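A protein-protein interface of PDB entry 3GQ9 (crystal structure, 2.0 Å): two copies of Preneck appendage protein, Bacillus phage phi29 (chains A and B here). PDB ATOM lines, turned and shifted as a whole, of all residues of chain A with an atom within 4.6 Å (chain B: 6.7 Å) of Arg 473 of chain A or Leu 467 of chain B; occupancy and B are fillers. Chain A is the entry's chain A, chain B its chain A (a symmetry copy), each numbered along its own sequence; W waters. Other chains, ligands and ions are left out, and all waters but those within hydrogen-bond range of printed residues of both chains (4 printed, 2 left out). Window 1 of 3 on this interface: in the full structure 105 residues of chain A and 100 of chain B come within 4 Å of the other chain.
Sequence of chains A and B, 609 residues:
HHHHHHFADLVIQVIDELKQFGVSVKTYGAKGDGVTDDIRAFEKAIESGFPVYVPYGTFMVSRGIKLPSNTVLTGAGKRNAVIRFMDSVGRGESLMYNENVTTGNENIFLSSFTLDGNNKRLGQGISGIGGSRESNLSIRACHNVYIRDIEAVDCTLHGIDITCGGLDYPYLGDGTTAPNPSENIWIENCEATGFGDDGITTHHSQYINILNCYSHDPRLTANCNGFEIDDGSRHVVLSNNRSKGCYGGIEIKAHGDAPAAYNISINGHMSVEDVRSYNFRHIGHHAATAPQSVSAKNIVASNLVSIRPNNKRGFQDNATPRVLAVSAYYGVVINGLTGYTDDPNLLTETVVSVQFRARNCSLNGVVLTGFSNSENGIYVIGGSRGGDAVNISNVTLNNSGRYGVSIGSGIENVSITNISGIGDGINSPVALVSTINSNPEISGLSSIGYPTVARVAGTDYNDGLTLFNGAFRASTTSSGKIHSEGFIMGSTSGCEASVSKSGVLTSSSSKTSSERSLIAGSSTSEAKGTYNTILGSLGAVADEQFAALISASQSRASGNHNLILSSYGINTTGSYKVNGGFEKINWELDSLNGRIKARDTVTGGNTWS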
ATOM      1  N   ALA A 471       2.465  29.897  29.968  1.00  0.00           N
ATOM      2  CA  ALA A 471       2.974  30.300  28.667  1.00  0.00           C
ATOM      3  C   ALA A 471       1.805  30.353  27.692  1.00  0.00           C
ATOM      4  O   ALA A 471       0.954  29.442  27.682  1.00  0.00           O
ATOM      5  CB  ALA A 471       4.017  29.306  28.209  1.00  0.00           C
ATOM      6  N   PHE A 472       1.726  31.427  26.904  1.00  0.00           N
ATOM      7  CA  PHE A 472       0.622  31.582  25.966  1.00  0.00           C
ATOM      8  C   PHE A 472       1.095  31.574  24.514  1.00  0.00           C
ATOM      9  O   PHE A 472       2.070  32.236  24.176  1.00  0.00           O
ATOM     10  CB  PHE A 472      -0.143  32.888  26.227  1.00  0.00           C
ATOM     11  CG  PHE A 472      -1.356  33.065  25.341  1.00  0.00           C
ATOM     12  CD1 PHE A 472      -2.483  32.256  25.500  1.00  0.00           C
ATOM     13  CD2 PHE A 472      -1.384  34.046  24.360  1.00  0.00           C
ATOM     14  CE1 PHE A 472      -3.612  32.414  24.676  1.00  0.00           C
ATOM     15  CE2 PHE A 472      -2.524  34.215  23.535  1.00  0.00           C
ATOM     16  CZ  PHE A 472      -3.627  33.387  23.701  1.00  0.00           C
ATOM     17  N   ARG A 473       0.361  30.880  23.652  1.00  0.00           N
ATOM     18  CA  ARG A 473       0.617  30.922  22.213  1.00  0.00           C
ATOM     19  C   ARG A 473      -0.689  30.865  21.439  1.00  0.00           C
ATOM     20  O   ARG A 473      -1.562  30.036  21.732  1.00  0.00           O
ATOM     21  CB  ARG A 473       1.528  29.763  21.782  1.00  0.00           C
ATOM     22  CG  ARG A 473       2.055  29.871  20.336  1.00  0.00           C
ATOM     23  CD  ARG A 473       2.965  28.690  19.991  1.00  0.00           C
ATOM     24  NE  ARG A 473       2.177  27.481  19.791  1.00  0.00           N
ATOM     25  CZ  ARG A 473       2.694  26.262  19.652  1.00  0.00           C
ATOM     26  NH1 ARG A 473       4.016  26.085  19.694  1.00  0.00           N
ATOM     27  NH2 ARG A 473       1.896  25.219  19.475  1.00  0.00           N
ATOM     28  N   ALA A 474      -0.813  31.747  20.451  1.00  0.00           N
ATOM     29  CA  ALA A 474      -1.980  31.765  19.562  1.00  0.00           C
ATOM     30  C   ALA A 474      -1.513  31.992  18.125  1.00  0.00           C
ATOM     31  O   ALA A 474      -0.448  32.563  17.905  1.00  0.00           O
ATOM     32  CB  ALA A 474      -2.975  32.850  19.983  1.00  0.00           C
ATOM     33  N   THR A 476      -0.028  30.391  15.899  1.00  0.00           N
ATOM     34  CA  THR A 476       1.351  29.970  15.646  1.00  0.00           C
ATOM     35  C   THR A 476       1.399  28.445  15.741  1.00  0.00           C
ATOM     36  O   THR A 476       1.201  27.888  16.819  1.00  0.00           O
ATOM     37  CB  THR A 476       2.320  30.577  16.694  1.00  0.00           C
ATOM     38  OG1 THR A 476       2.187  32.002  16.695  1.00  0.00           O
ATOM     39  CG2 THR A 476       3.789  30.213  16.399  1.00  0.00           C
ATOM     40  N   THR A 477       1.693  27.768  14.631  1.00  0.00           N
ATOM     41  CA  THR A 477       1.563  26.307  14.588  1.00  0.00           C
ATOM     42  C   THR A 477       2.707  25.543  15.268  1.00  0.00           C
ATOM     43  O   THR A 477       2.536  24.383  15.655  1.00  0.00           O
ATOM     44  CB  THR A 477       1.361  25.791  13.137  1.00  0.00           C
ATOM     45  OG1 THR A 477       2.513  26.123  12.377  1.00  0.00           O
ATOM     46  CG2 THR A 477       0.157  26.461  12.493  1.00  0.00           C
ATOM     47  N   SER A 478       3.871  26.176  15.389  1.00  0.00           N
ATOM     48  CA  SER A 478       4.981  25.606  16.147  1.00  0.00           C
ATOM     49  C   SER A 478       5.891  26.705  16.653  1.00  0.00           C
ATOM     50  O   SER A 478       5.960  27.786  16.073  1.00  0.00           O
ATOM     51  CB  SER A 478       5.803  24.603  15.327  1.00  0.00           C
ATOM     52  OG  SER A 478       6.347  25.223  14.196  1.00  0.00           O
ATOM     53  N   SER A 479       6.596  26.414  17.736  1.00  0.00           N
ATOM     54  CA  SER A 479       7.559  27.349  18.290  1.00  0.00           C
ATOM     55  C   SER A 479       8.529  26.581  19.171  1.00  0.00           C
ATOM     56  O   SER A 479       8.277  25.428  19.545  1.00  0.00           O
ATOM     57  CB  SER A 479       6.825  28.422  19.116  1.00  0.00           C
ATOM     58  OG  SER A 479       6.389  27.882  20.353  1.00  0.00           O
ATOM     59  N   ILE A 482       8.463  28.880  25.312  1.00  0.00           N
ATOM     60  CA  ILE A 482       7.793  30.112  25.759  1.00  0.00           C
ATOM     61  C   ILE A 482       7.735  30.084  27.288  1.00  0.00           C
ATOM     62  O   ILE A 482       7.234  29.126  27.883  1.00  0.00           O
ATOM     63  CB  ILE A 482       6.360  30.230  25.181  1.00  0.00           C
ATOM     64  CG1 ILE A 482       6.369  30.076  23.651  1.00  0.00           C
ATOM     65  CG2 ILE A 482       5.690  31.548  25.631  1.00  0.00           C
ATOM     66  CD1 ILE A 482       4.969  30.031  23.001  1.00  0.00           C
ATOM     67  N   ILE A 488       3.907  33.975  22.330  1.00  0.00           N
ATOM     68  CA  ILE A 488       4.188  34.113  20.904  1.00  0.00           C
ATOM     69  C   ILE A 488       2.826  34.126  20.212  1.00  0.00           C
ATOM     70  O   ILE A 488       1.987  33.259  20.487  1.00  0.00           O
ATOM     71  CB  ILE A 488       5.059  32.957  20.340  1.00  0.00           C
ATOM     72  CG1 ILE A 488       6.435  32.919  21.036  1.00  0.00           C
ATOM     73  CG2 ILE A 488       5.234  33.114  18.805  1.00  0.00           C
ATOM     74  CD1 ILE A 488       7.316  31.710  20.646  1.00  0.00           C
ATOM     75  N   SER B 438       3.082  19.418  16.825  1.00  0.00           N
ATOM     76  CA  SER B 438       3.550  20.660  17.429  1.00  0.00           C
ATOM     77  C   SER B 438       2.420  21.589  17.888  1.00  0.00           C
ATOM     78  O   SER B 438       2.646  22.477  18.720  1.00  0.00           O
ATOM     79  CB  SER B 438       4.507  21.380  16.473  1.00  0.00           C
ATOM     80  OG  SER B 438       3.814  21.877  15.326  1.00  0.00           O
ATOM     81  N   ASN B 439       1.206  21.346  17.387  1.00  0.00           N
ATOM     82  CA  ASN B 439       0.074  22.262  17.571  1.00  0.00           C
ATOM     83  C   ASN B 439      -1.156  21.692  18.313  1.00  0.00           C
ATOM     84  O   ASN B 439      -2.301  21.882  17.856  1.00  0.00           O
ATOM     85  CB  ASN B 439      -0.378  22.788  16.211  1.00  0.00           C
ATOM     86  CG  ASN B 439      -0.921  21.684  15.330  1.00  0.00           C
ATOM     87  OD1 ASN B 439      -0.522  20.511  15.461  1.00  0.00           O
ATOM     88  ND2 ASN B 439      -1.862  22.033  14.460  1.00  0.00           N
ATOM     89  N   PRO B 440      -0.946  21.051  19.475  1.00  0.00           N
ATOM     90  CA  PRO B 440      -2.116  20.642  20.237  1.00  0.00           C
ATOM     91  C   PRO B 440      -2.760  21.891  20.848  1.00  0.00           C
ATOM     92  O   PRO B 440      -2.070  22.888  21.077  1.00  0.00           O
ATOM     93  CB  PRO B 440      -1.497  19.797  21.356  1.00  0.00           C
ATOM     94  CG  PRO B 440      -0.161  20.465  21.600  1.00  0.00           C
ATOM     95  CD  PRO B 440       0.303  20.700  20.186  1.00  0.00           C
ATOM     96  N   GLU B 441      -4.061  21.852  21.103  1.00  0.00           N
ATOM     97  CA  GLU B 441      -4.672  22.888  21.932  1.00  0.00           C
ATOM     98  C   GLU B 441      -4.734  22.389  23.364  1.00  0.00           C
ATOM     99  O   GLU B 441      -5.252  21.292  23.632  1.00  0.00           O
ATOM    100  CB  GLU B 441      -6.053  23.288  21.402  1.00  0.00           C
ATOM    101  CG  GLU B 441      -5.955  23.953  20.012  1.00  0.00           C
ATOM    102  CD  GLU B 441      -7.271  24.576  19.565  1.00  0.00           C
ATOM    103  OE1 GLU B 441      -8.283  23.833  19.498  1.00  0.00           O
ATOM    104  OE2 GLU B 441      -7.298  25.801  19.298  1.00  0.00           O
ATOM    105  N   ILE B 442      -4.180  23.188  24.277  1.00  0.00           N
ATOM    106  CA  ILE B 442      -3.966  22.758  25.657  1.00  0.00           C
ATOM    107  C   ILE B 442      -4.262  23.889  26.624  1.00  0.00           C
ATOM    108  O   ILE B 442      -3.885  25.034  26.372  1.00  0.00           O
ATOM    109  CB  ILE B 442      -2.488  22.322  25.894  1.00  0.00           C
ATOM    110  CG1 ILE B 442      -2.127  21.083  25.047  1.00  0.00           C
ATOM    111  CG2 ILE B 442      -2.250  22.054  27.382  1.00  0.00           C
ATOM    112  CD1 ILE B 442      -0.642  20.586  25.213  1.00  0.00           C
ATOM    113  N   SER B 443      -4.929  23.571  27.727  1.00  0.00           N
ATOM    114  CA  SER B 443      -5.011  24.503  28.854  1.00  0.00           C
ATOM    115  C   SER B 443      -5.331  23.749  30.140  1.00  0.00           C
ATOM    116  O   SER B 443      -5.807  22.608  30.104  1.00  0.00           O
ATOM    117  CB  SER B 443      -6.077  25.581  28.590  1.00  0.00           C
ATOM    118  OG  SER B 443      -7.383  25.047  28.763  1.00  0.00           O
ATOM    119  N   VAL B 456       5.666  19.141  24.553  1.00  0.00           N
ATOM    120  CA  VAL B 456       5.001  19.388  23.275  1.00  0.00           C
ATOM    121  C   VAL B 456       6.048  19.309  22.185  1.00  0.00           C
ATOM    122  O   VAL B 456       6.921  20.174  22.094  1.00  0.00           O
ATOM    123  CB  VAL B 456       4.307  20.784  23.227  1.00  0.00           C
ATOM    124  CG1 VAL B 456       3.613  21.017  21.881  1.00  0.00           C
ATOM    125  CG2 VAL B 456       3.290  20.925  24.347  1.00  0.00           C
ATOM    126  N   TYR B 461       7.168  22.206  29.192  1.00  0.00           N
ATOM    127  CA  TYR B 461       6.451  23.294  29.838  1.00  0.00           C
ATOM    128  C   TYR B 461       6.043  22.819  31.213  1.00  0.00           C
ATOM    129  O   TYR B 461       5.179  21.941  31.339  1.00  0.00           O
ATOM    130  CB  TYR B 461       5.216  23.661  29.023  1.00  0.00           C
ATOM    131  CG  TYR B 461       5.567  24.352  27.737  1.00  0.00           C
ATOM    132  CD1 TYR B 461       5.786  23.627  26.566  1.00  0.00           C
ATOM    133  CD2 TYR B 461       5.709  25.731  27.700  1.00  0.00           C
ATOM    134  CE1 TYR B 461       6.128  24.265  25.392  1.00  0.00           C
ATOM    135  CE2 TYR B 461       6.055  26.380  26.546  1.00  0.00           C
ATOM    136  CZ  TYR B 461       6.266  25.650  25.392  1.00  0.00           C
ATOM    137  OH  TYR B 461       6.601  26.332  24.253  1.00  0.00           O
ATOM    138  N   LEU B 465       0.622  26.190  30.778  1.00  0.00           N
ATOM    139  CA  LEU B 465       0.544  26.576  29.378  1.00  0.00           C
ATOM    140  C   LEU B 465      -0.878  26.662  28.861  1.00  0.00           C
ATOM    141  O   LEU B 465      -1.771  25.915  29.289  1.00  0.00           O
ATOM    142  CB  LEU B 465       1.419  25.676  28.474  1.00  0.00           C
ATOM    143  CG  LEU B 465       0.883  24.405  27.834  1.00  0.00           C
ATOM    144  CD1 LEU B 465       1.879  23.813  26.824  1.00  0.00           C
ATOM    145  CD2 LEU B 465       0.635  23.402  28.940  1.00  0.00           C
ATOM    146  N   THR B 466      -1.062  27.602  27.939  1.00  0.00           N
ATOM    147  CA  THR B 466      -2.289  27.761  27.183  1.00  0.00           C
ATOM    148  C   THR B 466      -1.944  27.887  25.689  1.00  0.00           C
ATOM    149  O   THR B 466      -1.272  28.831  25.287  1.00  0.00           O
ATOM    150  CB  THR B 466      -3.062  29.016  27.637  1.00  0.00           C
ATOM    151  OG1 THR B 466      -3.383  28.892  29.031  1.00  0.00           O
ATOM    152  CG2 THR B 466      -4.360  29.145  26.834  1.00  0.00           C
ATOM    153  N   LEU B 467      -2.412  26.943  24.878  1.00  0.00           N
ATOM    154  CA  LEU B 467      -2.105  26.924  23.446  1.00  0.00           C
ATOM    155  C   LEU B 467      -3.405  26.870  22.655  1.00  0.00           C
ATOM    156  O   LEU B 467      -4.216  25.977  22.867  1.00  0.00           O
ATOM    157  CB  LEU B 467      -1.241  25.698  23.079  1.00  0.00           C
ATOM    158  CG  LEU B 467       0.093  25.453  23.804  1.00  0.00           C
ATOM    159  CD1 LEU B 467       0.724  24.165  23.241  1.00  0.00           C
ATOM    160  CD2 LEU B 467       1.046  26.621  23.643  1.00  0.00           C
ATOM    161  N   PHE B 468      -3.607  27.839  21.770  1.00  0.00           N
ATOM    162  CA  PHE B 468      -4.771  27.829  20.874  1.00  0.00           C
ATOM    163  C   PHE B 468      -4.331  27.910  19.421  1.00  0.00           C
ATOM    164  O   PHE B 468      -3.266  28.452  19.116  1.00  0.00           O
ATOM    165  CB  PHE B 468      -5.715  28.983  21.203  1.00  0.00           C
ATOM    166  CG  PHE B 468      -6.600  28.714  22.403  1.00  0.00           C
ATOM    167  CD1 PHE B 468      -6.298  29.270  23.645  1.00  0.00           C
ATOM    168  CD2 PHE B 468      -7.719  27.878  22.288  1.00  0.00           C
ATOM    169  CE1 PHE B 468      -7.098  29.017  24.746  1.00  0.00           C
ATOM    170  CE2 PHE B 468      -8.538  27.609  23.390  1.00  0.00           C
ATOM    171  CZ  PHE B 468      -8.225  28.190  24.625  1.00  0.00           C
ATOM    172  N   ASN B 469      -5.174  27.392  18.529  1.00  0.00           N
ATOM    173  CA  ASN B 469      -4.892  27.381  17.095  1.00  0.00           C
ATOM    174  C   ASN B 469      -5.799  28.305  16.282  1.00  0.00           C
ATOM    175  O   ASN B 469      -6.884  28.722  16.741  1.00  0.00           O
ATOM    176  CB  ASN B 469      -5.006  25.957  16.536  1.00  0.00           C
ATOM    177  CG  ASN B 469      -3.927  25.032  17.066  1.00  0.00           C
ATOM    178  OD1 ASN B 469      -2.926  25.481  17.630  1.00  0.00           O
ATOM    179  ND2 ASN B 469      -4.141  23.720  16.904  1.00  0.00           N
ATOM    180  N   PHE B 472      -6.631  34.341  15.704  1.00  0.00           N
ATOM    181  CA  PHE B 472      -6.940  34.654  17.094  1.00  0.00           C
ATOM    182  C   PHE B 472      -7.520  36.058  17.251  1.00  0.00           C
ATOM    183  O   PHE B 472      -7.002  37.011  16.679  1.00  0.00           O
ATOM    184  CB  PHE B 472      -5.687  34.535  17.975  1.00  0.00           C
ATOM    185  CG  PHE B 472      -5.959  34.764  19.445  1.00  0.00           C
ATOM    186  CD1 PHE B 472      -6.694  33.838  20.190  1.00  0.00           C
ATOM    187  CD2 PHE B 472      -5.474  35.892  20.093  1.00  0.00           C
ATOM    188  CE1 PHE B 472      -6.952  34.048  21.556  1.00  0.00           C
ATOM    189  CE2 PHE B 472      -5.724  36.100  21.472  1.00  0.00           C
ATOM    190  CZ  PHE B 472      -6.470  35.173  22.188  1.00  0.00           C
HETATM  191  O   HOH W   1       7.040  24.883  22.348  1.00  0.00           O
HETATM  192  O   HOH W   2      -0.656  27.565  19.975  1.00  0.00           O
HETATM  193  O   HOH W   3       5.089  23.619  19.192  1.00  0.00           O
HETATM  194  O   HOH W   4       6.951  22.701  21.013  1.00  0.00           O
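N of Phe 468 of chain B sits at hydrogen-bond distance from O of Arg 473 of chain A. The side-chain hydroxyl (OG) of Ser 438 of chain B sits at hydrogen-bond distance from the backbone carbonyl oxygen (O) of Thr 477 of chain A (2.8 Å). The backbone NH of Thr 466 of chain B lies within hydrogen-bond range of the backbone carbonyl oxygen of Ala 471 of chain A (2.7 Å). The backbone carbonyl oxygen (O) of Ser 438 of chain B is in hydrogen-bond range of the guanidinium group (NH2) of Arg 473 of chain A (2.9 Å). The backbone NH (N) of Ile 482 of chain A is in hydrogen-bond range of the side-chain hydroxyl (OH) of Tyr 461 of chain B (3.3 Å). The backbone NH (N) of Arg 473 of chain A sits at hydrogen-bond distance from the backbone carbonyl oxygen (O) of Thr 466 of chain B (3.1 Å).
The guanidinium group of Arg 473 of chain A lies within hydrogen-bond range of the backbone carbonyl oxygen of Thr 476 of chain A, 3.2 Å away. O of Ile 442 of chain B lies within hydrogen-bond range of N of Leu 467 of chain B. O of Asn 439 of chain B sits at hydrogen-bond distance from ND2 of Asn 469 of chain B (2.8 Å). The side-chain hydroxyl (OG1) of Thr 476 of chain A lies within hydrogen-bond range of the backbone carbonyl oxygen (O) of Ala 474 of chain A, at 3.0 Å. The guanidinium group (NH1) of Arg 473 of chain A sits at hydrogen-bond distance from the side-chain hydroxyl (OG) of Ser 479 of chain A (3.0 Å). N of Ile 488 of chain A lies within hydrogen-bond range of O of Phe 472 of chain A, 3.1 Å away.
CE2 of Tyr 461 of chain B touches CB of Ala 471 of chain A (3.9 Å). O of Ala 471 of chain A touches CA of Leu 465 of chain B, at 3.4 Å. Phe 472 of chain A touches Thr 466 of chain B. Phe 472 of chain B touches Phe 472 of chain A (CZ to CZ, 3.7 Å). NH2 of Arg 473 of chain A touches CA of Asn 439 of chain B, 3.96 Å away. CA of Leu 467 of chain B touches O of Arg 473 of chain A (3.6 Å). Ala 474 of chain A touches Phe 468 of chain B. Ala 474 of chain A touches Phe 472 of chain B (CB to CG, 3.6 Å). Thr 477 of chain A touches Asn 439 of chain B (O to CB, 3.4 Å). OG of Ser 438 of chain B touches CB of Ser 478 of chain A (3.4 Å).
Arg 473 of chain A touches five residues of chain B. Leu 467 of chain B touches one residue of chain A. Of the printed residues of chain B, Ala 474 of chain A touches Phe 468 and Phe 472. Printed residues of chain A within 4 Å of Tyr 461 of chain B: Ala 471 and Ile 482. The nearest residue of chain B that does not touch Arg 473 of chain A is Pro 440 of chain B (4.8 Å).
Printed residues of chain B that touch a printed residue of chain A: Ser 438, Asn 439, Tyr 461, Leu 465, Thr 466, Leu 467, Phe 468 and Phe 472. Hydrophobic or aromatic side chains of chain B that line the printed part of chain A: Tyr 461, Leu 465, Leu 467 and Phe 472. Printed residues of chain A that touch a printed residue of chain B: Ala 471, Phe 472, Arg 473, Ala 474, Thr 477, Ser 478 and Ile 482. Hydrophobic or aromatic side chains of chain A within 4 Å of the printed part of chain B: Ala 471, Phe 472, Ala 474 and Ile 482. Among the printed residues, 16 pairs touch across the chains.
Phe 472 of chain B touches its own counterpart, Phe 472 of chain A.
Water W1 bridges OH of Tyr 461 of chain B (2.4 Å) and O of Ser 479 of chain A (3.1 Å). Water W3 lies within hydrogen-bond range of NH1 of Arg 473 of chain A (2.7 Å), O of Ser 438 of chain B (2.7 Å) and N of Ser 479 of chain A (3.5 Å). Water W4 lies within hydrogen-bond range of the backbone carbonyl oxygen of Val 456 of chain B (2.7 Å) and the backbone carbonyl oxygen of Ser 479 of chain A (3.4 Å). Water W2 lies within hydrogen-bond range of the guanidinium group of Arg 473 of chain A and the backbone carbonyl oxygen of Phe 468 of chain B.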
